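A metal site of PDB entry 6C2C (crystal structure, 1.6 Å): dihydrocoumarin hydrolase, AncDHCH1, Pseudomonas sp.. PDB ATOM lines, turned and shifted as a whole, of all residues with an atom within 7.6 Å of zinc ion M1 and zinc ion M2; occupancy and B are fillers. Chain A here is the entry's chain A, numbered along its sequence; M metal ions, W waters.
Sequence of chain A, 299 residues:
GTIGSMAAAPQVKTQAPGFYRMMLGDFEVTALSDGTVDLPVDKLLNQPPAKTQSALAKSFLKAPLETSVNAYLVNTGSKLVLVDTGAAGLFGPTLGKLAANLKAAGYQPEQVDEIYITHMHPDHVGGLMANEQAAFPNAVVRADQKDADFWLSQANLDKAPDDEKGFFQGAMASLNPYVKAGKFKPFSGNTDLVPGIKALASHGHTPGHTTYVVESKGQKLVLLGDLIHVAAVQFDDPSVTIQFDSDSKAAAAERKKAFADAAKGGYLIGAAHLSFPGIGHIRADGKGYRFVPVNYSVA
A ring nitrogen (ND1) of His 205 is in hydrogen-bond range of the side-chain carboxylate of Asp 245. NE2 of His 209 sits at hydrogen-bond distance from N of Asp 226. ND1 of His 119 is in hydrogen-bond range of OG1 of Thr 118. A ring nitrogen (ND1) of His 124 sits at hydrogen-bond distance from the side-chain carboxylate of Asp 84 (2.8 Å). A ring nitrogen (ND1) of His 273 is in hydrogen-bond range of the backbone carbonyl oxygen (O) of Ser 68 (2.8 Å).
The nearest printed residue that does not touch zinc ion M1 is His 229 (4.7 Å).
Zinc ion M1 is bound by water W1 (1.9 Å). Zinc ion M1 is bound by a ring nitrogen (NE2) of His 124 (2.1 Å). OD2 of Asp 226 binds zinc ion M1 (2.1 Å). Zinc ion M1 is bound by NE2 of His 273 (2.2 Å). Zinc ion M1 is bound by OD2 of Asp 123 (2.3 Å). Zinc ion M1 has five donor atoms within binding distance.
Zinc ion M2 is bound by water W1 (1.9 Å), NE2 of His 119 (2.1 Å), OD2 of Asp 226 (2.2 Å), water W2 (2.2 Å), ND1 of His 121 (2.3 Å) and NE2 of His 205 (2.3 Å). Zinc ion M2 has six donor atoms within binding distance.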
ATOM      1  N   SER A  68      -7.985 -20.995   4.811  1.00  0.00           N
ATOM      2  CA  SER A  68      -8.428 -22.190   4.115  1.00  0.00           C
ATOM      3  C   SER A  68      -7.276 -23.110   3.785  1.00  0.00           C
ATOM      4  O   SER A  68      -6.155 -22.666   3.585  1.00  0.00           O
ATOM      5  CB  SER A  68      -9.102 -21.814   2.818  1.00  0.00           C
ATOM      6  OG  SER A  68     -10.379 -21.246   3.091  1.00  0.00           O
ATOM      7  N   VAL A  69      -7.597 -24.394   3.697  1.00  0.00           N
ATOM      8  CA  VAL A  69      -6.690 -25.431   3.236  1.00  0.00           C
ATOM      9  C   VAL A  69      -7.417 -26.177   2.140  1.00  0.00           C
ATOM     10  O   VAL A  69      -8.383 -26.911   2.424  1.00  0.00           O
ATOM     11  CB  VAL A  69      -6.266 -26.396   4.362  1.00  0.00           C
ATOM     12  CG1 VAL A  69      -5.300 -27.556   3.801  1.00  0.00           C
ATOM     13  CG2 VAL A  69      -5.522 -25.650   5.500  1.00  0.00           C
ATOM     14  N   ASN A  70      -6.955 -26.040   0.904  1.00  0.00           N
ATOM     15  CA  ASN A  70      -7.685 -26.558  -0.271  1.00  0.00           C
ATOM     16  C   ASN A  70      -6.881 -27.604  -1.015  1.00  0.00           C
ATOM     17  O   ASN A  70      -5.642 -27.592  -1.006  1.00  0.00           O
ATOM     18  CB  ASN A  70      -7.975 -25.446  -1.261  1.00  0.00           C
ATOM     19  CG  ASN A  70      -8.606 -24.185  -0.618  1.00  0.00           C
ATOM     20  OD1 ASN A  70      -9.439 -24.271   0.306  1.00  0.00           O
ATOM     21  ND2 ASN A  70      -8.225 -23.012  -1.129  1.00  0.00           N
ATOM     22  N   ASP A  84      -3.090 -32.409  -4.076  1.00  0.00           N
ATOM     23  CA  ASP A  84      -3.007 -32.242  -2.634  1.00  0.00           C
ATOM     24  C   ASP A  84      -4.114 -33.005  -1.886  1.00  0.00           C
ATOM     25  O   ASP A  84      -5.030 -33.411  -2.504  1.00  0.00           O
ATOM     26  CB  ASP A  84      -2.885 -30.820  -2.217  1.00  0.00           C
ATOM     27  CG  ASP A  84      -1.492 -30.240  -2.539  1.00  0.00           C
ATOM     28  OD1 ASP A  84      -0.577 -31.028  -2.806  1.00  0.00           O
ATOM     29  OD2 ASP A  84      -1.397 -29.027  -2.512  1.00  0.00           O
ATOM     30  N   THR A 118       1.833 -30.840  -4.148  1.00  0.00           N
ATOM     31  CA  THR A 118       2.605 -29.631  -4.447  1.00  0.00           C
ATOM     32  C   THR A 118       3.875 -29.563  -3.595  1.00  0.00           C
ATOM     33  O   THR A 118       4.933 -29.207  -4.094  1.00  0.00           O
ATOM     34  CB  THR A 118       1.741 -28.363  -4.212  1.00  0.00           C
ATOM     35  OG1 THR A 118       1.290 -28.319  -2.836  1.00  0.00           O
ATOM     36  CG2 THR A 118       0.563 -28.304  -5.199  1.00  0.00           C
ATOM     37  N   HIS A 119       3.773 -30.000  -2.346  1.00  0.00           N
ATOM     38  CA  HIS A 119       4.916 -30.058  -1.444  1.00  0.00           C
ATOM     39  C   HIS A 119       4.511 -30.861  -0.217  1.00  0.00           C
ATOM     40  O   HIS A 119       3.325 -31.015   0.075  1.00  0.00           O
ATOM     41  CB  HIS A 119       5.389 -28.655  -1.043  1.00  0.00           C
ATOM     42  CG  HIS A 119       4.406 -27.843  -0.245  1.00  0.00           C
ATOM     43  ND1 HIS A 119       3.147 -27.486  -0.705  1.00  0.00           N
ATOM     44  CD2 HIS A 119       4.534 -27.268   0.983  1.00  0.00           C
ATOM     45  CE1 HIS A 119       2.537 -26.745   0.209  1.00  0.00           C
ATOM     46  NE2 HIS A 119       3.365 -26.556   1.238  1.00  0.00           N
ATOM     47  N   MET A 120       5.528 -31.391   0.487  1.00  0.00           N
ATOM     48  CA  MET A 120       5.202 -32.344   1.570  1.00  0.00           C
ATOM     49  C   MET A 120       5.011 -31.719   2.938  1.00  0.00           C
ATOM     50  O   MET A 120       5.286 -32.358   3.943  1.00  0.00           O
ATOM     51  CB  MET A 120       6.264 -33.438   1.621  1.00  0.00           C
ATOM     52  CG  MET A 120       6.256 -34.237   0.292  1.00  0.00           C
ATOM     53  SD  MET A 120       7.399 -35.657   0.416  1.00  0.00           S
ATOM     54  CE  MET A 120       7.145 -36.309  -1.246  1.00  0.00           C
ATOM     55  N   HIS A 121       4.407 -30.552   3.042  1.00  0.00           N
ATOM     56  CA  HIS A 121       3.955 -30.061   4.318  1.00  0.00           C
ATOM     57  C   HIS A 121       2.743 -30.840   4.789  1.00  0.00           C
ATOM     58  O   HIS A 121       2.029 -31.468   3.991  1.00  0.00           O
ATOM     59  CB  HIS A 121       3.642 -28.561   4.206  1.00  0.00           C
ATOM     60  CG  HIS A 121       4.859 -27.688   4.255  1.00  0.00           C
ATOM     61  ND1 HIS A 121       4.870 -26.358   3.932  1.00  0.00           N
ATOM     62  CD2 HIS A 121       6.149 -27.978   4.595  1.00  0.00           C
ATOM     63  CE1 HIS A 121       6.078 -25.833   4.070  1.00  0.00           C
ATOM     64  NE2 HIS A 121       6.875 -26.805   4.484  1.00  0.00           N
ATOM     65  N   PRO A 122       2.497 -30.857   6.094  1.00  0.00           N
ATOM     66  CA  PRO A 122       1.491 -31.767   6.643  1.00  0.00           C
ATOM     67  C   PRO A 122       0.102 -31.528   6.139  1.00  0.00           C
ATOM     68  O   PRO A 122      -0.649 -32.481   6.012  1.00  0.00           O
ATOM     69  CB  PRO A 122       1.549 -31.500   8.154  1.00  0.00           C
ATOM     70  CG  PRO A 122       2.152 -30.177   8.252  1.00  0.00           C
ATOM     71  CD  PRO A 122       3.204 -30.140   7.161  1.00  0.00           C
ATOM     72  N   ASP A 123      -0.239 -30.289   5.842  1.00  0.00           N
ATOM     73  CA  ASP A 123      -1.567 -29.922   5.362  1.00  0.00           C
ATOM     74  C   ASP A 123      -1.715 -30.182   3.888  1.00  0.00           C
ATOM     75  O   ASP A 123      -2.775 -29.889   3.333  1.00  0.00           O
ATOM     76  CB  ASP A 123      -1.858 -28.449   5.653  1.00  0.00           C
ATOM     77  CG  ASP A 123      -0.745 -27.466   5.113  1.00  0.00           C
ATOM     78  OD1 ASP A 123       0.464 -27.652   5.243  1.00  0.00           O
ATOM     79  OD2 ASP A 123      -1.141 -26.485   4.553  1.00  0.00           O
ATOM     80  N   HIS A 124      -0.741 -30.845   3.263  1.00  0.00           N
ATOM     81  CA  HIS A 124      -0.909 -31.301   1.881  1.00  0.00           C
ATOM     82  C   HIS A 124      -0.777 -32.802   1.702  1.00  0.00           C
ATOM     83  O   HIS A 124      -1.399 -33.363   0.778  1.00  0.00           O
ATOM     84  CB  HIS A 124       0.098 -30.598   0.957  1.00  0.00           C
ATOM     85  CG  HIS A 124      -0.060 -29.087   1.069  1.00  0.00           C
ATOM     86  ND1 HIS A 124      -0.729 -28.320   0.136  1.00  0.00           N
ATOM     87  CD2 HIS A 124       0.280 -28.250   2.088  1.00  0.00           C
ATOM     88  CE1 HIS A 124      -0.787 -27.069   0.570  1.00  0.00           C
ATOM     89  NE2 HIS A 124      -0.190 -27.010   1.766  1.00  0.00           N
ATOM     90  N   PHE A 167       7.075 -32.046  10.971  1.00  0.00           N
ATOM     91  CA  PHE A 167       6.863 -31.953   9.535  1.00  0.00           C
ATOM     92  C   PHE A 167       7.451 -33.177   8.834  1.00  0.00           C
ATOM     93  O   PHE A 167       6.834 -33.765   7.929  1.00  0.00           O
ATOM     94  CB  PHE A 167       7.490 -30.683   8.957  1.00  0.00           C
ATOM     95  CG  PHE A 167       6.728 -29.441   9.274  1.00  0.00           C
ATOM     96  CD1 PHE A 167       5.881 -29.394  10.382  1.00  0.00           C
ATOM     97  CD2 PHE A 167       6.855 -28.326   8.448  1.00  0.00           C
ATOM     98  CE1 PHE A 167       5.155 -28.248  10.677  1.00  0.00           C
ATOM     99  CE2 PHE A 167       6.136 -27.155   8.743  1.00  0.00           C
ATOM    100  CZ  PHE A 167       5.296 -27.127   9.865  1.00  0.00           C
ATOM    101  N   HIS A 205       9.290 -22.427  -1.508  1.00  0.00           N
ATOM    102  CA  HIS A 205       8.505 -22.680  -0.300  1.00  0.00           C
ATOM    103  C   HIS A 205       8.991 -23.979   0.397  1.00  0.00           C
ATOM    104  O   HIS A 205       9.035 -24.067   1.572  1.00  0.00           O
ATOM    105  CB  HIS A 205       7.032 -22.738  -0.633  1.00  0.00           C
ATOM    106  CG  HIS A 205       6.166 -23.007   0.532  1.00  0.00           C
ATOM    107  ND1 HIS A 205       6.040 -22.136   1.584  1.00  0.00           N
ATOM    108  CD2 HIS A 205       5.382 -24.052   0.818  1.00  0.00           C
ATOM    109  CE1 HIS A 205       5.207 -22.650   2.460  1.00  0.00           C
ATOM    110  NE2 HIS A 205       4.812 -23.809   2.023  1.00  0.00           N
ATOM    111  N   THR A 206       9.280 -24.955  -0.460  1.00  0.00           N
ATOM    112  CA  THR A 206      10.047 -26.135  -0.075  1.00  0.00           C
ATOM    113  C   THR A 206      11.008 -26.433  -1.221  1.00  0.00           C
ATOM    114  O   THR A 206      10.778 -25.972  -2.336  1.00  0.00           O
ATOM    115  CB  THR A 206       9.139 -27.346   0.193  1.00  0.00           C
ATOM    116  OG1 THR A 206       8.532 -27.762  -1.049  1.00  0.00           O
ATOM    117  CG2 THR A 206       8.093 -27.039   1.260  1.00  0.00           C
ATOM    118  N   HIS A 209       8.913 -27.675  -4.190  1.00  0.00           N
ATOM    119  CA  HIS A 209       7.553 -27.187  -4.353  1.00  0.00           C
ATOM    120  C   HIS A 209       7.218 -27.108  -5.847  1.00  0.00           C
ATOM    121  O   HIS A 209       8.014 -26.622  -6.657  1.00  0.00           O
ATOM    122  CB  HIS A 209       7.390 -25.815  -3.673  1.00  0.00           C
ATOM    123  CG  HIS A 209       5.972 -25.306  -3.732  1.00  0.00           C
ATOM    124  ND1 HIS A 209       5.452 -24.734  -4.886  1.00  0.00           N
ATOM    125  CD2 HIS A 209       4.962 -25.344  -2.828  1.00  0.00           C
ATOM    126  CE1 HIS A 209       4.168 -24.426  -4.651  1.00  0.00           C
ATOM    127  NE2 HIS A 209       3.862 -24.778  -3.420  1.00  0.00           N
ATOM    128  N   GLY A 225      -0.289 -24.345  -5.297  1.00  0.00           N
ATOM    129  CA  GLY A 225       0.206 -24.871  -4.007  1.00  0.00           C
ATOM    130  C   GLY A 225       0.254 -23.752  -2.994  1.00  0.00           C
ATOM    131  O   GLY A 225      -0.725 -23.016  -2.808  1.00  0.00           O
ATOM    132  N   ASP A 226       1.402 -23.607  -2.373  1.00  0.00           N
ATOM    133  CA  ASP A 226       1.631 -22.567  -1.396  1.00  0.00           C
ATOM    134  C   ASP A 226       2.507 -21.354  -1.830  1.00  0.00           C
ATOM    135  O   ASP A 226       3.333 -20.884  -1.102  1.00  0.00           O
ATOM    136  CB  ASP A 226       2.206 -23.191  -0.129  1.00  0.00           C
ATOM    137  CG  ASP A 226       1.181 -23.941   0.707  1.00  0.00           C
ATOM    138  OD1 ASP A 226       0.137 -24.192   0.286  1.00  0.00           O
ATOM    139  OD2 ASP A 226       1.552 -24.288   1.763  1.00  0.00           O
ATOM    140  N   LEU A 227       2.360 -20.968  -3.073  1.00  0.00           N
ATOM    141  CA  LEU A 227       2.988 -19.709  -3.493  1.00  0.00           C
ATOM    142  C   LEU A 227       2.387 -18.503  -2.788  1.00  0.00           C
ATOM    143  O   LEU A 227       2.941 -17.418  -2.889  1.00  0.00           O
ATOM    144  CB  LEU A 227       2.895 -19.510  -5.009  1.00  0.00           C
ATOM    145  CG  LEU A 227       3.627 -20.483  -5.931  1.00  0.00           C
ATOM    146  CD1 LEU A 227       3.754 -19.979  -7.372  1.00  0.00           C
ATOM    147  CD2 LEU A 227       4.989 -20.968  -5.385  1.00  0.00           C
ATOM    148  N   ILE A 228       1.253 -18.645  -2.078  1.00  0.00           N
ATOM    149  CA  ILE A 228       0.695 -17.534  -1.324  1.00  0.00           C
ATOM    150  C   ILE A 228       0.071 -18.092  -0.047  1.00  0.00           C
ATOM    151  O   ILE A 228      -0.433 -19.220  -0.032  1.00  0.00           O
ATOM    152  CB  ILE A 228      -0.296 -16.730  -2.187  1.00  0.00           C
ATOM    153  CG1 ILE A 228      -0.900 -15.514  -1.435  1.00  0.00           C
ATOM    154  CG2 ILE A 228      -1.409 -17.631  -2.637  1.00  0.00           C
ATOM    155  CD1 ILE A 228      -1.220 -14.304  -2.379  1.00  0.00           C
ATOM    156  N   HIS A 229       0.146 -17.326   1.063  1.00  0.00           N
ATOM    157  CA  HIS A 229      -0.525 -17.693   2.293  1.00  0.00           C
ATOM    158  C   HIS A 229      -1.527 -16.673   2.774  1.00  0.00           C
ATOM    159  O   HIS A 229      -2.474 -17.052   3.482  1.00  0.00           O
ATOM    160  CB  HIS A 229       0.444 -17.934   3.457  1.00  0.00           C
ATOM    161  CG  HIS A 229       1.272 -19.171   3.281  1.00  0.00           C
ATOM    162  ND1 HIS A 229       2.331 -19.222   2.385  1.00  0.00           N
ATOM    163  CD2 HIS A 229       1.182 -20.388   3.853  1.00  0.00           C
ATOM    164  CE1 HIS A 229       2.862 -20.426   2.439  1.00  0.00           C
ATOM    165  NE2 HIS A 229       2.215 -21.147   3.336  1.00  0.00           N
ATOM    166  N   ILE A 242       7.037 -15.711   4.319  1.00  0.00           N
ATOM    167  CA  ILE A 242       6.489 -16.281   5.545  1.00  0.00           C
ATOM    168  C   ILE A 242       7.489 -17.277   6.126  1.00  0.00           C
ATOM    169  O   ILE A 242       8.309 -17.870   5.402  1.00  0.00           O
ATOM    170  CB  ILE A 242       5.090 -16.917   5.260  1.00  0.00           C
ATOM    171  CG1 ILE A 242       4.295 -17.204   6.537  1.00  0.00           C
ATOM    172  CG2 ILE A 242       5.196 -18.207   4.367  1.00  0.00           C
ATOM    173  CD1 ILE A 242       2.745 -17.364   6.189  1.00  0.00           C
ATOM    174  N   PHE A 244       7.064 -20.193   7.054  1.00  0.00           N
ATOM    175  CA  PHE A 244       6.919 -21.546   6.546  1.00  0.00           C
ATOM    176  C   PHE A 244       7.787 -21.815   5.308  1.00  0.00           C
ATOM    177  O   PHE A 244       7.912 -22.966   4.918  1.00  0.00           O
ATOM    178  CB  PHE A 244       5.457 -21.823   6.170  1.00  0.00           C
ATOM    179  CG  PHE A 244       4.480 -21.678   7.297  1.00  0.00           C
ATOM    180  CD1 PHE A 244       4.761 -22.188   8.558  1.00  0.00           C
ATOM    181  CD2 PHE A 244       3.242 -21.037   7.065  1.00  0.00           C
ATOM    182  CE1 PHE A 244       3.837 -22.080   9.576  1.00  0.00           C
ATOM    183  CE2 PHE A 244       2.325 -20.926   8.089  1.00  0.00           C
ATOM    184  CZ  PHE A 244       2.622 -21.470   9.330  1.00  0.00           C
ATOM    185  N   ASP A 245       8.292 -20.796   4.635  1.00  0.00           N
ATOM    186  CA  ASP A 245       9.121 -20.999   3.449  1.00  0.00           C
ATOM    187  C   ASP A 245      10.462 -21.603   3.829  1.00  0.00           C
ATOM    188  O   ASP A 245      11.141 -21.067   4.714  1.00  0.00           O
ATOM    189  CB  ASP A 245       9.403 -19.675   2.730  1.00  0.00           C
ATOM    190  CG  ASP A 245       8.151 -19.047   2.132  1.00  0.00           C
ATOM    191  OD1 ASP A 245       7.249 -19.756   1.638  1.00  0.00           O
ATOM    192  OD2 ASP A 245       8.091 -17.796   2.119  1.00  0.00           O
ATOM    193  N   ALA A 272      -3.827 -23.299  -2.496  1.00  0.00           N
ATOM    194  CA  ALA A 272      -4.183 -24.069  -1.289  1.00  0.00           C
ATOM    195  C   ALA A 272      -4.647 -23.199  -0.121  1.00  0.00           C
ATOM    196  O   ALA A 272      -5.481 -23.667   0.678  1.00  0.00           O
ATOM    197  CB  ALA A 272      -2.970 -24.890  -0.809  1.00  0.00           C
ATOM    198  N   HIS A 273      -4.174 -21.926  -0.029  1.00  0.00           N
ATOM    199  CA  HIS A 273      -4.496 -21.099   1.150  1.00  0.00           C
ATOM    200  C   HIS A 273      -5.177 -19.794   0.764  1.00  0.00           C
ATOM    201  O   HIS A 273      -5.209 -18.863   1.578  1.00  0.00           O
ATOM    202  CB  HIS A 273      -3.226 -20.840   2.012  1.00  0.00           C
ATOM    203  CG  HIS A 273      -2.641 -22.148   2.522  1.00  0.00           C
ATOM    204  ND1 HIS A 273      -3.413 -23.125   3.126  1.00  0.00           N
ATOM    205  CD2 HIS A 273      -1.401 -22.640   2.434  1.00  0.00           C
ATOM    206  CE1 HIS A 273      -2.644 -24.171   3.412  1.00  0.00           C
ATOM    207  NE2 HIS A 273      -1.430 -23.908   3.002  1.00  0.00           N
HETATM  208 ZN    ZN M   1       0.182 -25.358   3.012  1.00  0.00          ZN
HETATM  209 ZN    ZN M   2       3.186 -25.220   2.893  1.00  0.00          ZN
HETATM  210  O   HOH W   1       1.729 -25.822   3.930  1.00  0.00           O
HETATM  211  O   HOH W   2       3.247 -23.575   4.399  1.00  0.00           O
